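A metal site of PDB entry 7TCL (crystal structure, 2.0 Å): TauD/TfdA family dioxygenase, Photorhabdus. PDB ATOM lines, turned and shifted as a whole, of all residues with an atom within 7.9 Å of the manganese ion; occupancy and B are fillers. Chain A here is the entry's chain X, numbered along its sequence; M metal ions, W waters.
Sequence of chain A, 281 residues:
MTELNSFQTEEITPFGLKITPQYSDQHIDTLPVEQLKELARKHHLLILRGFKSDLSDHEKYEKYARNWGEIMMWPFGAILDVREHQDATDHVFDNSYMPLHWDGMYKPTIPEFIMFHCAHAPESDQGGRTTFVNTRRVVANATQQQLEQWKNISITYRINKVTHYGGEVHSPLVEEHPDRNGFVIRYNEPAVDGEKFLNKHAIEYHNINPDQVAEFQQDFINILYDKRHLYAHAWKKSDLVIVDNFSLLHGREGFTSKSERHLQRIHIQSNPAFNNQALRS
ND1 of His 101 is in hydrogen-bond range of O of Pro 99 (2.8 Å). NH1 of Arg 265 is in salt-bridge range of OD2 of Asp 103 (3.9 Å). The side-chain carboxylate (OD2) of Asp 103 is in hydrogen-bond range of a ring nitrogen (NE2) of His 267 (2.6 Å). O of Asp 103 is in hydrogen-bond range of ND2 of Asn 245, at 2.9 Å.
Within 4 Å of the manganese ion: His 101, Asp 103 and His 250.
The manganese ion is bound by NE2 of His 250 (2.2 Å), OD1 of Asp 103 (2.2 Å), water W2 (2.3 Å), NE2 of His 101 (2.3 Å), water W3 (2.3 Å) and water W1 (2.4 Å). The manganese ion has six donor atoms within binding distance.
Water W2 bridges OD2 of Asp 103 (2.8 Å) and NH1 of Arg 265 (3.4 Å).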
ATOM      1  N   LEU A  80     -35.045  30.421  16.931  1.00  0.00           N
ATOM      2  CA  LEU A  80     -35.013  29.183  17.692  1.00  0.00           C
ATOM      3  C   LEU A  80     -35.131  29.519  19.172  1.00  0.00           C
ATOM      4  O   LEU A  80     -34.359  30.342  19.673  1.00  0.00           O
ATOM      5  CB  LEU A  80     -33.741  28.381  17.428  1.00  0.00           C
ATOM      6  CG  LEU A  80     -33.606  27.096  18.267  1.00  0.00           C
ATOM      7  CD1 LEU A  80     -34.614  26.056  17.802  1.00  0.00           C
ATOM      8  CD2 LEU A  80     -32.190  26.532  18.193  1.00  0.00           C
ATOM      9  N   VAL A  82     -34.342  28.214  22.603  1.00  0.00           N
ATOM     10  CA  VAL A  82     -33.489  27.226  23.246  1.00  0.00           C
ATOM     11  C   VAL A  82     -33.938  27.122  24.695  1.00  0.00           C
ATOM     12  O   VAL A  82     -33.823  28.081  25.471  1.00  0.00           O
ATOM     13  CB  VAL A  82     -32.004  27.596  23.142  1.00  0.00           C
ATOM     14  CG1 VAL A  82     -31.129  26.539  23.799  1.00  0.00           C
ATOM     15  CG2 VAL A  82     -31.610  27.778  21.671  1.00  0.00           C
ATOM     16  N   MET A  98     -22.449  20.623  25.757  1.00  0.00           N
ATOM     17  CA  MET A  98     -22.681  20.580  24.336  1.00  0.00           C
ATOM     18  C   MET A  98     -21.384  20.882  23.584  1.00  0.00           C
ATOM     19  O   MET A  98     -20.723  21.901  23.859  1.00  0.00           O
ATOM     20  CB  MET A  98     -23.793  21.510  23.898  1.00  0.00           C
ATOM     21  CG  MET A  98     -23.982  21.279  22.386  1.00  0.00           C
ATOM     22  SD  MET A  98     -25.549  21.767  21.615  1.00  0.00           S
ATOM     23  CE  MET A  98     -25.575  23.483  21.943  1.00  0.00           C
ATOM     24  N   PRO A  99     -20.986  20.005  22.646  1.00  0.00           N
ATOM     25  CA  PRO A  99     -19.662  20.120  22.008  1.00  0.00           C
ATOM     26  C   PRO A  99     -19.506  21.411  21.229  1.00  0.00           C
ATOM     27  O   PRO A  99     -20.458  21.938  20.648  1.00  0.00           O
ATOM     28  CB  PRO A  99     -19.619  18.915  21.061  1.00  0.00           C
ATOM     29  CG  PRO A  99     -20.680  17.968  21.581  1.00  0.00           C
ATOM     30  CD  PRO A  99     -21.738  18.818  22.191  1.00  0.00           C
ATOM     31  N   LEU A 100     -18.281  21.897  21.204  1.00  0.00           N
ATOM     32  CA  LEU A 100     -17.926  22.994  20.303  1.00  0.00           C
ATOM     33  C   LEU A 100     -18.302  22.650  18.873  1.00  0.00           C
ATOM     34  O   LEU A 100     -18.135  21.518  18.424  1.00  0.00           O
ATOM     35  CB  LEU A 100     -16.426  23.280  20.407  1.00  0.00           C
ATOM     36  CG  LEU A 100     -15.905  23.813  21.747  1.00  0.00           C
ATOM     37  CD1 LEU A 100     -14.366  24.009  21.673  1.00  0.00           C
ATOM     38  CD2 LEU A 100     -16.604  25.137  22.130  1.00  0.00           C
ATOM     39  N   HIS A 101     -18.825  23.642  18.164  1.00  0.00           N
ATOM     40  CA  HIS A 101     -19.189  23.516  16.756  1.00  0.00           C
ATOM     41  C   HIS A 101     -19.310  24.919  16.187  1.00  0.00           C
ATOM     42  O   HIS A 101     -19.182  25.914  16.910  1.00  0.00           O
ATOM     43  CB  HIS A 101     -20.516  22.737  16.601  1.00  0.00           C
ATOM     44  CG  HIS A 101     -21.659  23.399  17.296  1.00  0.00           C
ATOM     45  ND1 HIS A 101     -21.831  23.323  18.662  1.00  0.00           N
ATOM     46  CD2 HIS A 101     -22.654  24.185  16.825  1.00  0.00           C
ATOM     47  CE1 HIS A 101     -22.908  24.016  19.004  1.00  0.00           C
ATOM     48  NE2 HIS A 101     -23.436  24.533  17.910  1.00  0.00           N
ATOM     49  N   TRP A 102     -19.535  25.013  14.887  1.00  0.00           N
ATOM     50  CA  TRP A 102     -19.993  26.250  14.292  1.00  0.00           C
ATOM     51  C   TRP A 102     -21.417  26.050  13.771  1.00  0.00           C
ATOM     52  O   TRP A 102     -21.847  24.917  13.521  1.00  0.00           O
ATOM     53  CB  TRP A 102     -19.033  26.718  13.197  1.00  0.00           C
ATOM     54  CG  TRP A 102     -18.991  25.905  11.913  1.00  0.00           C
ATOM     55  CD1 TRP A 102     -19.481  26.281  10.696  1.00  0.00           C
ATOM     56  CD2 TRP A 102     -18.371  24.617  11.701  1.00  0.00           C
ATOM     57  NE1 TRP A 102     -19.243  25.305   9.755  1.00  0.00           N
ATOM     58  CE2 TRP A 102     -18.551  24.281  10.344  1.00  0.00           C
ATOM     59  CE3 TRP A 102     -17.703  23.704  12.528  1.00  0.00           C
ATOM     60  CZ2 TRP A 102     -18.083  23.088   9.794  1.00  0.00           C
ATOM     61  CZ3 TRP A 102     -17.248  22.519  11.992  1.00  0.00           C
ATOM     62  CH2 TRP A 102     -17.438  22.219  10.634  1.00  0.00           C
ATOM     63  N   ASP A 103     -22.191  27.135  13.704  1.00  0.00           N
ATOM     64  CA  ASP A 103     -23.578  27.023  13.284  1.00  0.00           C
ATOM     65  C   ASP A 103     -23.670  26.974  11.760  1.00  0.00           C
ATOM     66  O   ASP A 103     -22.889  27.609  11.053  1.00  0.00           O
ATOM     67  CB  ASP A 103     -24.428  28.188  13.822  1.00  0.00           C
ATOM     68  CG  ASP A 103     -24.976  27.944  15.230  1.00  0.00           C
ATOM     69  OD1 ASP A 103     -24.650  26.890  15.821  1.00  0.00           O
ATOM     70  OD2 ASP A 103     -25.736  28.792  15.748  1.00  0.00           O
ATOM     71  N   GLY A 104     -24.640  26.207  11.266  1.00  0.00           N
ATOM     72  CA  GLY A 104     -24.825  26.059   9.830  1.00  0.00           C
ATOM     73  C   GLY A 104     -24.176  24.824   9.219  1.00  0.00           C
ATOM     74  O   GLY A 104     -24.308  24.617   8.010  1.00  0.00           O
ATOM     75  N   ILE A 114     -24.475  34.994  14.939  1.00  0.00           N
ATOM     76  CA  ILE A 114     -25.514  34.440  15.804  1.00  0.00           C
ATOM     77  C   ILE A 114     -25.939  35.529  16.774  1.00  0.00           C
ATOM     78  O   ILE A 114     -25.090  36.159  17.424  1.00  0.00           O
ATOM     79  CB  ILE A 114     -25.026  33.208  16.585  1.00  0.00           C
ATOM     80  CG1 ILE A 114     -24.212  32.264  15.715  1.00  0.00           C
ATOM     81  CG2 ILE A 114     -26.228  32.468  17.183  1.00  0.00           C
ATOM     82  CD1 ILE A 114     -23.465  31.189  16.515  1.00  0.00           C
ATOM     83  N   PHE A 116     -28.115  35.843  20.191  1.00  0.00           N
ATOM     84  CA  PHE A 116     -28.760  35.159  21.314  1.00  0.00           C
ATOM     85  C   PHE A 116     -29.369  36.226  22.215  1.00  0.00           C
ATOM     86  O   PHE A 116     -28.672  37.113  22.699  1.00  0.00           O
ATOM     87  CB  PHE A 116     -27.763  34.343  22.141  1.00  0.00           C
ATOM     88  CG  PHE A 116     -27.286  33.082  21.460  1.00  0.00           C
ATOM     89  CD1 PHE A 116     -28.125  32.000  21.306  1.00  0.00           C
ATOM     90  CD2 PHE A 116     -25.982  32.981  21.012  1.00  0.00           C
ATOM     91  CE1 PHE A 116     -27.673  30.824  20.717  1.00  0.00           C
ATOM     92  CE2 PHE A 116     -25.518  31.820  20.411  1.00  0.00           C
ATOM     93  CZ  PHE A 116     -26.363  30.742  20.264  1.00  0.00           C
ATOM     94  N   ASN A 245     -19.874  33.974  13.980  1.00  0.00           N
ATOM     95  CA  ASN A 245     -19.883  32.535  13.671  1.00  0.00           C
ATOM     96  C   ASN A 245     -18.796  32.125  12.697  1.00  0.00           C
ATOM     97  O   ASN A 245     -18.442  30.938  12.626  1.00  0.00           O
ATOM     98  CB  ASN A 245     -21.272  32.125  13.138  1.00  0.00           C
ATOM     99  CG  ASN A 245     -21.415  30.622  12.961  1.00  0.00           C
ATOM    100  OD1 ASN A 245     -21.168  29.838  13.874  1.00  0.00           O
ATOM    101  ND2 ASN A 245     -21.839  30.205  11.777  1.00  0.00           N
ATOM    102  N   LEU A 249     -15.934  29.102  17.460  1.00  0.00           N
ATOM    103  CA  LEU A 249     -16.738  27.934  17.782  1.00  0.00           C
ATOM    104  C   LEU A 249     -17.456  28.210  19.097  1.00  0.00           C
ATOM    105  O   LEU A 249     -17.014  29.052  19.885  1.00  0.00           O
ATOM    106  CB  LEU A 249     -15.871  26.682  17.910  1.00  0.00           C
ATOM    107  CG  LEU A 249     -14.968  26.360  16.702  1.00  0.00           C
ATOM    108  CD1 LEU A 249     -14.027  25.226  17.053  1.00  0.00           C
ATOM    109  CD2 LEU A 249     -15.798  26.000  15.466  1.00  0.00           C
ATOM    110  N   HIS A 250     -18.571  27.520  19.322  1.00  0.00           N
ATOM    111  CA  HIS A 250     -19.331  27.733  20.545  1.00  0.00           C
ATOM    112  C   HIS A 250     -19.974  26.427  21.004  1.00  0.00           C
ATOM    113  O   HIS A 250     -20.166  25.482  20.223  1.00  0.00           O
ATOM    114  CB  HIS A 250     -20.399  28.826  20.380  1.00  0.00           C
ATOM    115  CG  HIS A 250     -21.500  28.419  19.463  1.00  0.00           C
ATOM    116  ND1 HIS A 250     -21.358  28.428  18.092  1.00  0.00           N
ATOM    117  CD2 HIS A 250     -22.736  27.928  19.716  1.00  0.00           C
ATOM    118  CE1 HIS A 250     -22.470  27.976  17.543  1.00  0.00           C
ATOM    119  NE2 HIS A 250     -23.322  27.675  18.497  1.00  0.00           N
ATOM    120  N   GLY A 251     -20.294  26.370  22.296  1.00  0.00           N
ATOM    121  CA  GLY A 251     -20.811  25.157  22.907  1.00  0.00           C
ATOM    122  C   GLY A 251     -21.451  25.468  24.245  1.00  0.00           C
ATOM    123  O   GLY A 251     -21.902  26.590  24.453  1.00  0.00           O
ATOM    124  N   ARG A 265     -32.561  32.566  19.559  1.00  0.00           N
ATOM    125  CA  ARG A 265     -31.440  32.641  18.624  1.00  0.00           C
ATOM    126  C   ARG A 265     -31.913  33.022  17.231  1.00  0.00           C
ATOM    127  O   ARG A 265     -32.832  32.409  16.684  1.00  0.00           O
ATOM    128  CB  ARG A 265     -30.715  31.294  18.573  1.00  0.00           C
ATOM    129  CG  ARG A 265     -29.482  31.283  17.657  1.00  0.00           C
ATOM    130  CD  ARG A 265     -29.117  29.846  17.206  1.00  0.00           C
ATOM    131  NE  ARG A 265     -30.028  29.380  16.175  1.00  0.00           N
ATOM    132  CZ  ARG A 265     -30.089  28.119  15.734  1.00  0.00           C
ATOM    133  NH1 ARG A 265     -29.292  27.184  16.251  1.00  0.00           N
ATOM    134  NH2 ARG A 265     -30.959  27.802  14.788  1.00  0.00           N
ATOM    135  N   HIS A 267     -30.126  33.840  13.282  1.00  0.00           N
ATOM    136  CA  HIS A 267     -28.939  33.828  12.428  1.00  0.00           C
ATOM    137  C   HIS A 267     -29.034  34.911  11.357  1.00  0.00           C
ATOM    138  O   HIS A 267     -30.080  35.063  10.708  1.00  0.00           O
ATOM    139  CB  HIS A 267     -28.776  32.469  11.718  1.00  0.00           C
ATOM    140  CG  HIS A 267     -28.332  31.355  12.613  1.00  0.00           C
ATOM    141  ND1 HIS A 267     -28.816  30.063  12.477  1.00  0.00           N
ATOM    142  CD2 HIS A 267     -27.420  31.304  13.611  1.00  0.00           C
ATOM    143  CE1 HIS A 267     -28.233  29.282  13.373  1.00  0.00           C
ATOM    144  NE2 HIS A 267     -27.382  30.010  14.073  1.00  0.00           N
HETATM  145 MN    MN M   1     -24.902  26.298  17.915  1.00  0.00          MN
HETATM  146  O   HOH W   1     -25.526  25.798  20.187  1.00  0.00           O
HETATM  147  O   HOH W   2     -26.589  27.806  18.197  1.00  0.00           O
HETATM  148  O   HOH W   3     -26.607  24.960  17.020  1.00  0.00           O
